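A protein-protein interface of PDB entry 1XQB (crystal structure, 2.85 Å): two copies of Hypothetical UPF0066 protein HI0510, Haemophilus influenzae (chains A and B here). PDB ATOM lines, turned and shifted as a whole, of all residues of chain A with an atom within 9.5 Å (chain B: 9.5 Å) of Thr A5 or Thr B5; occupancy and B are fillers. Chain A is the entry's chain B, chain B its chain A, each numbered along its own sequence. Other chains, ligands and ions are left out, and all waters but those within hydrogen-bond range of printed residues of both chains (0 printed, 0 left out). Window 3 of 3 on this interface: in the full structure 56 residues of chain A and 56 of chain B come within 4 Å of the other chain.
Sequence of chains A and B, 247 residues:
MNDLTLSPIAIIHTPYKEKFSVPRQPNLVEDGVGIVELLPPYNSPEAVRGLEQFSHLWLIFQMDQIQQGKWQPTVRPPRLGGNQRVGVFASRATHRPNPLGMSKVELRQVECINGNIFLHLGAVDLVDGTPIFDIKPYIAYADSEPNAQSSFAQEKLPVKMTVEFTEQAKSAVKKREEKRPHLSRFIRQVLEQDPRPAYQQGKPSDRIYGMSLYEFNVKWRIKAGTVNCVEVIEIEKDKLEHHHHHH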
ATOM      1  N   ASN A   2       5.089  22.832   3.593  1.00  0.00           N
ATOM      2  CA  ASN A   2       4.663  21.494   3.994  1.00  0.00           C
ATOM      3  C   ASN A   2       5.723  20.833   4.881  1.00  0.00           C
ATOM      4  O   ASN A   2       6.634  21.502   5.366  1.00  0.00           O
ATOM      5  CB  ASN A   2       4.401  20.638   2.742  1.00  0.00           C
ATOM      6  CG  ASN A   2       3.402  21.286   1.777  1.00  0.00           C
ATOM      7  OD1 ASN A   2       2.269  21.616   2.153  1.00  0.00           O
ATOM      8  ND2 ASN A   2       3.826  21.474   0.529  1.00  0.00           N
ATOM      9  N   ASP A   3       5.600  19.524   5.084  1.00  0.00           N
ATOM     10  CA  ASP A   3       6.541  18.757   5.899  1.00  0.00           C
ATOM     11  C   ASP A   3       7.942  18.730   5.285  1.00  0.00           C
ATOM     12  O   ASP A   3       8.253  19.518   4.397  1.00  0.00           O
ATOM     13  CB  ASP A   3       6.045  17.312   6.069  1.00  0.00           C
ATOM     14  CG  ASP A   3       4.789  17.208   6.918  1.00  0.00           C
ATOM     15  OD1 ASP A   3       3.925  16.370   6.589  1.00  0.00           O
ATOM     16  OD2 ASP A   3       4.673  17.941   7.918  1.00  0.00           O
ATOM     17  N   LEU A   4       8.786  17.827   5.779  1.00  0.00           N
ATOM     18  CA  LEU A   4      10.151  17.673   5.279  1.00  0.00           C
ATOM     19  C   LEU A   4      10.705  16.318   5.719  1.00  0.00           C
ATOM     20  O   LEU A   4      10.596  15.939   6.893  1.00  0.00           O
ATOM     21  CB  LEU A   4      11.063  18.796   5.794  1.00  0.00           C
ATOM     22  CG  LEU A   4      12.504  18.765   5.263  1.00  0.00           C
ATOM     23  CD1 LEU A   4      12.547  19.279   3.829  1.00  0.00           C
ATOM     24  CD2 LEU A   4      13.405  19.600   6.134  1.00  0.00           C
ATOM     25  N   THR A   5      11.277  15.580   4.772  1.00  0.00           N
ATOM     26  CA  THR A   5      11.842  14.275   5.082  1.00  0.00           C
ATOM     27  C   THR A   5      13.371  14.342   5.127  1.00  0.00           C
ATOM     28  O   THR A   5      14.034  14.703   4.152  1.00  0.00           O
ATOM     29  CB  THR A   5      11.338  13.178   4.100  1.00  0.00           C
ATOM     30  OG1 THR A   5       9.933  12.962   4.301  1.00  0.00           O
ATOM     31  CG2 THR A   5      12.066  11.856   4.343  1.00  0.00           C
ATOM     32  N   LEU A   6      13.912  13.995   6.291  1.00  0.00           N
ATOM     33  CA  LEU A   6      15.343  14.013   6.539  1.00  0.00           C
ATOM     34  C   LEU A   6      16.016  12.672   6.324  1.00  0.00           C
ATOM     35  O   LEU A   6      15.512  11.636   6.741  1.00  0.00           O
ATOM     36  CB  LEU A   6      15.605  14.416   7.979  1.00  0.00           C
ATOM     37  CG  LEU A   6      14.983  15.689   8.495  1.00  0.00           C
ATOM     38  CD1 LEU A   6      15.346  15.831   9.953  1.00  0.00           C
ATOM     39  CD2 LEU A   6      15.512  16.855   7.677  1.00  0.00           C
ATOM     40  N   SER A   7      17.205  12.715   5.740  1.00  0.00           N
ATOM     41  CA  SER A   7      17.993  11.515   5.505  1.00  0.00           C
ATOM     42  C   SER A   7      19.263  11.592   6.361  1.00  0.00           C
ATOM     43  O   SER A   7      19.991  12.583   6.325  1.00  0.00           O
ATOM     44  CB  SER A   7      18.342  11.392   4.021  1.00  0.00           C
ATOM     45  OG  SER A   7      18.779  12.635   3.511  1.00  0.00           O
ATOM     46  N   PRO A   8      19.519  10.560   7.176  1.00  0.00           N
ATOM     47  CA  PRO A   8      20.718  10.574   8.019  1.00  0.00           C
ATOM     48  C   PRO A   8      21.953  10.644   7.135  1.00  0.00           C
ATOM     49  O   PRO A   8      22.075   9.867   6.193  1.00  0.00           O
ATOM     50  CB  PRO A   8      20.642   9.225   8.729  1.00  0.00           C
ATOM     51  CG  PRO A   8      19.171   8.891   8.716  1.00  0.00           C
ATOM     52  CD  PRO A   8      18.753   9.312   7.353  1.00  0.00           C
ATOM     53  N   TYR A  42      27.285  10.774   1.011  1.00  0.00           N
ATOM     54  CA  TYR A  42      27.761  12.043   1.553  1.00  0.00           C
ATOM     55  C   TYR A  42      29.212  11.970   1.997  1.00  0.00           C
ATOM     56  O   TYR A  42      29.862  12.990   2.197  1.00  0.00           O
ATOM     57  CB  TYR A  42      26.872  12.469   2.718  1.00  0.00           C
ATOM     58  CG  TYR A  42      25.384  12.236   2.476  1.00  0.00           C
ATOM     59  CD1 TYR A  42      24.705  11.224   3.139  1.00  0.00           C
ATOM     60  CD2 TYR A  42      24.669  13.038   1.593  1.00  0.00           C
ATOM     61  CE1 TYR A  42      23.365  11.020   2.936  1.00  0.00           C
ATOM     62  CE2 TYR A  42      23.320  12.846   1.375  1.00  0.00           C
ATOM     63  CZ  TYR A  42      22.668  11.835   2.053  1.00  0.00           C
ATOM     64  OH  TYR A  42      21.310  11.645   1.860  1.00  0.00           O
ATOM     65  N   GLN A  62      19.543  13.001  15.947  1.00  0.00           N
ATOM     66  CA  GLN A  62      18.211  12.501  16.274  1.00  0.00           C
ATOM     67  C   GLN A  62      18.158  12.119  17.753  1.00  0.00           C
ATOM     68  O   GLN A  62      19.052  11.451  18.262  1.00  0.00           O
ATOM     69  CB  GLN A  62      17.872  11.285  15.406  1.00  0.00           C
ATOM     70  CG  GLN A  62      16.385  11.015  15.306  1.00  0.00           C
ATOM     71  CD  GLN A  62      16.080   9.625  14.796  1.00  0.00           C
ATOM     72  OE1 GLN A  62      15.807   8.726  15.585  1.00  0.00           O
ATOM     73  NE2 GLN A  62      16.138   9.432  13.472  1.00  0.00           N
ATOM     74  N   ARG A  96       9.917  15.715  21.593  1.00  0.00           N
ATOM     75  CA  ARG A  96       9.543  16.934  20.884  1.00  0.00           C
ATOM     76  C   ARG A  96       8.798  16.654  19.595  1.00  0.00           C
ATOM     77  O   ARG A  96       8.875  15.549  19.045  1.00  0.00           O
ATOM     78  CB  ARG A  96      10.780  17.731  20.525  1.00  0.00           C
ATOM     79  CG  ARG A  96      11.464  18.305  21.682  1.00  0.00           C
ATOM     80  CD  ARG A  96      12.648  19.047  21.224  1.00  0.00           C
ATOM     81  NE  ARG A  96      13.239  19.757  22.339  1.00  0.00           N
ATOM     82  CZ  ARG A  96      12.769  20.901  22.810  1.00  0.00           C
ATOM     83  NH1 ARG A  96      11.700  21.454  22.258  1.00  0.00           N
ATOM     84  NH2 ARG A  96      13.386  21.510  23.809  1.00  0.00           N
ATOM     85  N   PRO A  97       8.046  17.656  19.100  1.00  0.00           N
ATOM     86  CA  PRO A  97       7.283  17.529  17.856  1.00  0.00           C
ATOM     87  C   PRO A  97       8.253  17.131  16.759  1.00  0.00           C
ATOM     88  O   PRO A  97       7.884  16.465  15.801  1.00  0.00           O
ATOM     89  CB  PRO A  97       6.746  18.936  17.655  1.00  0.00           C
ATOM     90  CG  PRO A  97       6.483  19.379  19.067  1.00  0.00           C
ATOM     91  CD  PRO A  97       7.727  18.923  19.791  1.00  0.00           C
ATOM     92  N   ASN A  98       9.502  17.549  16.932  1.00  0.00           N
ATOM     93  CA  ASN A  98      10.605  17.226  16.026  1.00  0.00           C
ATOM     94  C   ASN A  98      11.785  16.927  16.959  1.00  0.00           C
ATOM     95  O   ASN A  98      12.359  17.827  17.578  1.00  0.00           O
ATOM     96  CB  ASN A  98      10.903  18.390  15.083  1.00  0.00           C
ATOM     97  CG  ASN A  98       9.812  18.593  14.046  1.00  0.00           C
ATOM     98  OD1 ASN A  98       9.413  17.661  13.348  1.00  0.00           O
ATOM     99  ND2 ASN A  98       9.318  19.812  13.950  1.00  0.00           N
ATOM    100  N   PRO A  99      12.123  15.637  17.115  1.00  0.00           N
ATOM    101  CA  PRO A  99      13.225  15.238  17.997  1.00  0.00           C
ATOM    102  C   PRO A  99      14.623  15.633  17.496  1.00  0.00           C
ATOM    103  O   PRO A  99      15.567  14.844  17.565  1.00  0.00           O
ATOM    104  CB  PRO A  99      13.023  13.723  18.107  1.00  0.00           C
ATOM    105  CG  PRO A  99      12.515  13.369  16.733  1.00  0.00           C
ATOM    106  CD  PRO A  99      11.527  14.467  16.438  1.00  0.00           C
ATOM    107  N   LEU A 100      14.762  16.880  17.056  1.00  0.00           N
ATOM    108  CA  LEU A 100      16.040  17.371  16.556  1.00  0.00           C
ATOM    109  C   LEU A 100      16.907  17.997  17.635  1.00  0.00           C
ATOM    110  O   LEU A 100      16.568  19.025  18.213  1.00  0.00           O
ATOM    111  CB  LEU A 100      15.834  18.364  15.415  1.00  0.00           C
ATOM    112  CG  LEU A 100      15.225  17.795  14.135  1.00  0.00           C
ATOM    113  CD1 LEU A 100      14.957  18.934  13.187  1.00  0.00           C
ATOM    114  CD2 LEU A 100      16.126  16.758  13.497  1.00  0.00           C
ATOM    115  N   PHE A 133      22.032  14.379  11.391  1.00  0.00           N
ATOM    116  CA  PHE A 133      21.266  14.992  10.316  1.00  0.00           C
ATOM    117  C   PHE A 133      22.029  16.080   9.589  1.00  0.00           C
ATOM    118  O   PHE A 133      21.823  16.282   8.399  1.00  0.00           O
ATOM    119  CB  PHE A 133      19.939  15.533  10.833  1.00  0.00           C
ATOM    120  CG  PHE A 133      18.970  14.461  11.206  1.00  0.00           C
ATOM    121  CD1 PHE A 133      18.360  14.459  12.455  1.00  0.00           C
ATOM    122  CD2 PHE A 133      18.659  13.449  10.295  1.00  0.00           C
ATOM    123  CE1 PHE A 133      17.451  13.476  12.801  1.00  0.00           C
ATOM    124  CE2 PHE A 133      17.745  12.450  10.626  1.00  0.00           C
ATOM    125  CZ  PHE A 133      17.136  12.467  11.888  1.00  0.00           C
ATOM    126  N   ASN B   2      16.312   4.896  10.280  1.00  0.00           N
ATOM    127  CA  ASN B   2      15.720   5.270   9.000  1.00  0.00           C
ATOM    128  C   ASN B   2      15.569   6.791   8.896  1.00  0.00           C
ATOM    129  O   ASN B   2      16.143   7.530   9.693  1.00  0.00           O
ATOM    130  CB  ASN B   2      14.352   4.586   8.846  1.00  0.00           C
ATOM    131  CG  ASN B   2      14.428   3.068   9.015  1.00  0.00           C
ATOM    132  OD1 ASN B   2      15.191   2.387   8.323  1.00  0.00           O
ATOM    133  ND2 ASN B   2      13.635   2.538   9.943  1.00  0.00           N
ATOM    134  N   ASP B   3      14.790   7.250   7.919  1.00  0.00           N
ATOM    135  CA  ASP B   3      14.551   8.675   7.708  1.00  0.00           C
ATOM    136  C   ASP B   3      13.783   9.310   8.870  1.00  0.00           C
ATOM    137  O   ASP B   3      13.685   8.733   9.945  1.00  0.00           O
ATOM    138  CB  ASP B   3      13.768   8.894   6.409  1.00  0.00           C
ATOM    139  CG  ASP B   3      14.576   8.563   5.163  1.00  0.00           C
ATOM    140  OD1 ASP B   3      13.999   7.966   4.229  1.00  0.00           O
ATOM    141  OD2 ASP B   3      15.776   8.910   5.101  1.00  0.00           O
ATOM    142  N   LEU B   4      13.260  10.513   8.649  1.00  0.00           N
ATOM    143  CA  LEU B   4      12.487  11.230   9.658  1.00  0.00           C
ATOM    144  C   LEU B   4      11.666  12.331   8.989  1.00  0.00           C
ATOM    145  O   LEU B   4      12.185  13.103   8.175  1.00  0.00           O
ATOM    146  CB  LEU B   4      13.404  11.841  10.726  1.00  0.00           C
ATOM    147  CG  LEU B   4      12.695  12.554  11.891  1.00  0.00           C
ATOM    148  CD1 LEU B   4      12.127  11.537  12.866  1.00  0.00           C
ATOM    149  CD2 LEU B   4      13.654  13.460  12.618  1.00  0.00           C
ATOM    150  N   THR B   5      10.377  12.387   9.314  1.00  0.00           N
ATOM    151  CA  THR B   5       9.505  13.401   8.739  1.00  0.00           C
ATOM    152  C   THR B   5       9.207  14.504   9.753  1.00  0.00           C
ATOM    153  O   THR B   5       8.652  14.263  10.826  1.00  0.00           O
ATOM    154  CB  THR B   5       8.201  12.789   8.178  1.00  0.00           C
ATOM    155  OG1 THR B   5       8.510  11.963   7.046  1.00  0.00           O
ATOM    156  CG2 THR B   5       7.236  13.888   7.742  1.00  0.00           C
ATOM    157  N   LEU B   6       9.598  15.720   9.389  1.00  0.00           N
ATOM    158  CA  LEU B   6       9.418  16.892  10.232  1.00  0.00           C
ATOM    159  C   LEU B   6       8.156  17.679   9.933  1.00  0.00           C
ATOM    160  O   LEU B   6       7.823  17.924   8.777  1.00  0.00           O
ATOM    161  CB  LEU B   6      10.591  17.843  10.048  1.00  0.00           C
ATOM    162  CG  LEU B   6      12.005  17.325  10.203  1.00  0.00           C
ATOM    163  CD1 LEU B   6      12.957  18.460   9.908  1.00  0.00           C
ATOM    164  CD2 LEU B   6      12.191  16.810  11.614  1.00  0.00           C
ATOM    165  N   SER B   7       7.500  18.138  10.991  1.00  0.00           N
ATOM    166  CA  SER B   7       6.296  18.948  10.861  1.00  0.00           C
ATOM    167  C   SER B   7       6.603  20.362  11.369  1.00  0.00           C
ATOM    168  O   SER B   7       7.123  20.544  12.469  1.00  0.00           O
ATOM    169  CB  SER B   7       5.149  18.319  11.651  1.00  0.00           C
ATOM    170  OG  SER B   7       5.584  17.929  12.942  1.00  0.00           O
ATOM    171  N   PRO B   8       6.329  21.382  10.546  1.00  0.00           N
ATOM    172  CA  PRO B   8       6.602  22.756  10.974  1.00  0.00           C
ATOM    173  C   PRO B   8       5.763  23.075  12.202  1.00  0.00           C
ATOM    174  O   PRO B   8       4.562  22.830  12.200  1.00  0.00           O
ATOM    175  CB  PRO B   8       6.139  23.580   9.776  1.00  0.00           C
ATOM    176  CG  PRO B   8       6.252  22.616   8.610  1.00  0.00           C
ATOM    177  CD  PRO B   8       5.737  21.348   9.195  1.00  0.00           C
ATOM    178  N   TYR B  42       0.526  23.057  18.399  1.00  0.00           N
ATOM    179  CA  TYR B  42       1.674  23.324  19.268  1.00  0.00           C
ATOM    180  C   TYR B  42       1.560  24.659  19.993  1.00  0.00           C
ATOM    181  O   TYR B  42       2.256  24.911  20.966  1.00  0.00           O
ATOM    182  CB  TYR B  42       2.962  23.281  18.444  1.00  0.00           C
ATOM    183  CG  TYR B  42       3.006  22.145  17.441  1.00  0.00           C
ATOM    184  CD1 TYR B  42       2.882  22.397  16.082  1.00  0.00           C
ATOM    185  CD2 TYR B  42       3.182  20.829  17.854  1.00  0.00           C
ATOM    186  CE1 TYR B  42       2.938  21.376  15.152  1.00  0.00           C
ATOM    187  CE2 TYR B  42       3.233  19.788  16.943  1.00  0.00           C
ATOM    188  CZ  TYR B  42       3.115  20.067  15.582  1.00  0.00           C
ATOM    189  OH  TYR B  42       3.205  19.047  14.648  1.00  0.00           O
ATOM    190  N   GLN B  62      13.805  26.060   8.282  1.00  0.00           N
ATOM    191  CA  GLN B  62      13.989  25.476   6.957  1.00  0.00           C
ATOM    192  C   GLN B  62      14.699  26.475   6.036  1.00  0.00           C
ATOM    193  O   GLN B  62      14.330  27.640   5.959  1.00  0.00           O
ATOM    194  CB  GLN B  62      12.639  25.083   6.356  1.00  0.00           C
ATOM    195  CG  GLN B  62      12.745  24.041   5.264  1.00  0.00           C
ATOM    196  CD  GLN B  62      11.498  23.948   4.412  1.00  0.00           C
ATOM    197  OE1 GLN B  62      11.450  24.525   3.329  1.00  0.00           O
ATOM    198  NE2 GLN B  62      10.476  23.228   4.895  1.00  0.00           N
ATOM    199  N   ARG B  96      21.814  21.805   1.227  1.00  0.00           N
ATOM    200  CA  ARG B  96      22.304  20.713   2.053  1.00  0.00           C
ATOM    201  C   ARG B  96      21.445  19.466   1.954  1.00  0.00           C
ATOM    202  O   ARG B  96      20.276  19.534   1.557  1.00  0.00           O
ATOM    203  CB  ARG B  96      22.334  21.140   3.507  1.00  0.00           C
ATOM    204  CG  ARG B  96      23.342  22.165   3.808  1.00  0.00           C
ATOM    205  CD  ARG B  96      23.279  22.487   5.245  1.00  0.00           C
ATOM    206  NE  ARG B  96      24.373  23.358   5.601  1.00  0.00           N
ATOM    207  CZ  ARG B  96      25.616  22.938   5.776  1.00  0.00           C
ATOM    208  NH1 ARG B  96      25.909  21.657   5.621  1.00  0.00           N
ATOM    209  NH2 ARG B  96      26.557  23.789   6.138  1.00  0.00           N
ATOM    210  N   PRO B  97      22.025  18.301   2.298  1.00  0.00           N
ATOM    211  CA  PRO B  97      21.315  17.018   2.264  1.00  0.00           C
ATOM    212  C   PRO B  97      20.069  17.157   3.119  1.00  0.00           C
ATOM    213  O   PRO B  97      19.057  16.502   2.892  1.00  0.00           O
ATOM    214  CB  PRO B  97      22.323  16.074   2.895  1.00  0.00           C
ATOM    215  CG  PRO B  97      23.627  16.623   2.390  1.00  0.00           C
ATOM    216  CD  PRO B  97      23.459  18.105   2.581  1.00  0.00           C
ATOM    217  N   ASN B  98      20.170  18.031   4.116  1.00  0.00           N
ATOM    218  CA  ASN B  98      19.074  18.357   5.027  1.00  0.00           C
ATOM    219  C   ASN B  98      19.189  19.875   5.210  1.00  0.00           C
ATOM    220  O   ASN B  98      20.101  20.378   5.873  1.00  0.00           O
ATOM    221  CB  ASN B  98      19.217  17.601   6.350  1.00  0.00           C
ATOM    222  CG  ASN B  98      18.967  16.105   6.196  1.00  0.00           C
ATOM    223  OD1 ASN B  98      17.974  15.680   5.603  1.00  0.00           O
ATOM    224  ND2 ASN B  98      19.871  15.307   6.727  1.00  0.00           N
ATOM    225  N   PRO B  99      18.287  20.631   4.566  1.00  0.00           N
ATOM    226  CA  PRO B  99      18.314  22.094   4.655  1.00  0.00           C
ATOM    227  C   PRO B  99      17.928  22.657   6.024  1.00  0.00           C
ATOM    228  O   PRO B  99      17.173  23.631   6.110  1.00  0.00           O
ATOM    229  CB  PRO B  99      17.351  22.509   3.544  1.00  0.00           C
ATOM    230  CG  PRO B  99      16.310  21.403   3.590  1.00  0.00           C
ATOM    231  CD  PRO B  99      17.149  20.160   3.748  1.00  0.00           C
ATOM    232  N   LEU B 100      18.486  22.076   7.085  1.00  0.00           N
ATOM    233  CA  LEU B 100      18.195  22.526   8.443  1.00  0.00           C
ATOM    234  C   LEU B 100      19.134  23.618   8.932  1.00  0.00           C
ATOM    235  O   LEU B 100      20.324  23.397   9.107  1.00  0.00           O
ATOM    236  CB  LEU B 100      18.211  21.361   9.427  1.00  0.00           C
ATOM    237  CG  LEU B 100      17.129  20.303   9.240  1.00  0.00           C
ATOM    238  CD1 LEU B 100      17.374  19.202  10.233  1.00  0.00           C
ATOM    239  CD2 LEU B 100      15.745  20.878   9.409  1.00  0.00           C
ATOM    240  N   PHE B 133      11.188  24.559  12.727  1.00  0.00           N
ATOM    241  CA  PHE B 133      11.117  23.148  13.078  1.00  0.00           C
ATOM    242  C   PHE B 133      11.238  22.902  14.566  1.00  0.00           C
ATOM    243  O   PHE B 133      10.661  21.954  15.083  1.00  0.00           O
ATOM    244  CB  PHE B 133      12.165  22.339  12.329  1.00  0.00           C
ATOM    245  CG  PHE B 133      11.888  22.222  10.871  1.00  0.00           C
ATOM    246  CD1 PHE B 133      12.859  22.544   9.936  1.00  0.00           C
ATOM    247  CD2 PHE B 133      10.648  21.776  10.429  1.00  0.00           C
ATOM    248  CE1 PHE B 133      12.608  22.424   8.583  1.00  0.00           C
ATOM    249  CE2 PHE B 133      10.379  21.648   9.064  1.00  0.00           C
ATOM    250  CZ  PHE B 133      11.368  21.974   8.141  1.00  0.00           C
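Of the printed residues of chain B, Thr A5 touches Asp B3, Leu B4 and Thr B5.
Printed residues of chain A within 4 Å of Thr B5: Asp A3 (3.99 Å), Leu A4 (3.3 Å) and Thr A5 (3.2 Å).
Leu A4 touches just these residues of chain B: Leu B4, Thr B5, Leu B6 and Phe B133.
Leu A6 touches just these residues of chain B: Asp B3 (3.2 Å), Leu B4 (2.7 Å), Leu B6 (3.6 Å), Asn B98 (3.3 Å) and Leu B100 (3.9 Å).
Of chain A, only Leu A4, Thr A5, Leu A6 and Phe A133 come within 4 Å of Leu B4.
Of the printed residues of chain B, Asn A2 touches Pro B8.
Of the printed residues of chain A, Leu B100 touches Leu A6 (3.9 Å) and Leu A100 (3.8 Å).
Printed residues of chain A within 4 Å of Tyr B42: Pro A97 (3.7 Å).
Of the printed residues of chain A, Asn B2 touches Pro A8.
Of the printed residues of chain A, Leu B6 touches Asp A3 (3.3 Å), Leu A4 (2.7 Å), Leu A6 (3.6 Å), Asn A98 (3.2 Å) and Leu A100 (3.8 Å).
Arg B96 touches none of the printed residues of chain A.
The nearest printed residue of chain A that does not touch Thr B5 is Asn A98 (4.3 Å).
Among the printed residues, pairs that only touch across the chains: Asn A98 with Leu B6 (3.2 Å), Leu A6 with Asn B98 (3.3 Å), Leu A4 with Thr B5 (3.3 Å), Thr A5 with Leu B4 (3.3 Å), Ser A7 with Asp B3 (3.4 Å), Asn A2 with Pro B8 (3.5 Å), Pro A8 with Asn B2 (3.5 Å), Asp A3 with Ser B7 (3.5 Å), Leu A6 with Leu B6 (3.6 Å), Pro A97 with Tyr B42 (3.7 Å), Phe A133 with Leu B4 (3.7 Å), Tyr A42 with Pro B97 (3.7 Å), Leu A4 with Phe B133 (3.7 Å), Pro A8 with Asp B3 (3.8 Å), Asp A3 with Pro B8 (3.8 Å), Leu A100 with Leu B6 (3.8 Å), Leu A100 with Leu B100 (3.8 Å), Ser A7 with Pro B97 (3.9 Å), Leu A6 with Leu B100 (3.9 Å), Pro A97 with Ser B7 (3.95 Å), Thr A5 with Asp B3 (3.99 Å) and Asp A3 with Thr B5 (3.99 Å).
The backbone NH (N) of Leu A6 sits at hydrogen-bond distance from the backbone carbonyl oxygen (O) of Leu B4 (2.7 Å).
The side-chain hydroxyl (OG1) of Thr B5 lies within hydrogen-bond range of the side-chain hydroxyl (OG1) of Thr A5 (3.2 Å).
N of Leu B6 sits at hydrogen-bond distance from O of Leu A4, at 2.7 Å.
The side-chain amide nitrogen (ND2) of Asn A98 is in hydrogen-bond range of the backbone carbonyl oxygen (O) of Ser B7 (2.7 Å).
The side-chain amide nitrogen (ND2) of Asn B98 lies within hydrogen-bond range of the backbone carbonyl oxygen (O) of Ser A7, 2.8 Å away.
ND2 of Asn B98 is in hydrogen-bond range of O of Phe A133, at 2.7 Å.
O of Phe B133 sits at hydrogen-bond distance from ND2 of Asn A98.
OD2 of Asp A3 lies close to O of Leu B6 (3.3 Å).
The backbone carbonyl oxygen (O) of Leu A4 lies close to the backbone carbonyl oxygen (O) of Leu B4 (3.5 Å).
OD2 of Asp B3 lies close to O of Leu A6.
Hydrophobic or aromatic side chains of chain A that line the printed part of chain B: Leu A4, Leu A6, Pro A8, Tyr A42, Pro A97, Leu A100 and Phe A133.
Among the printed residues, 32 pairs touch across the chains.
Among the printed residues, no Asp or Glu carboxylate lies within 4 Å of a Lys or Arg side-chain nitrogen of the other chain.
Asp A3 touches Thr B5, and with the chains exchanged Thr A5 touches Asp B3.
Asp A3 touches Pro B8, and with the chains exchanged Pro A8 touches Asp B3.
Leu A4 touches Phe B133, and with the chains exchanged Phe A133 touches Leu B4.
Leu A100 touches its own counterpart, Leu B100.
Positions printed for both chains: 2, 3, 4, 5, 6, 7, 8, 42, 62, 96, 97, 98, 99, 100 and 133.
OH of Tyr B42 sits at hydrogen-bond distance from OG of Ser B7, 3.1 Å away.
The side-chain hydroxyl (OG) of Ser A7 lies within hydrogen-bond range of the side-chain hydroxyl (OH) of Tyr A42 (3.2 Å).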
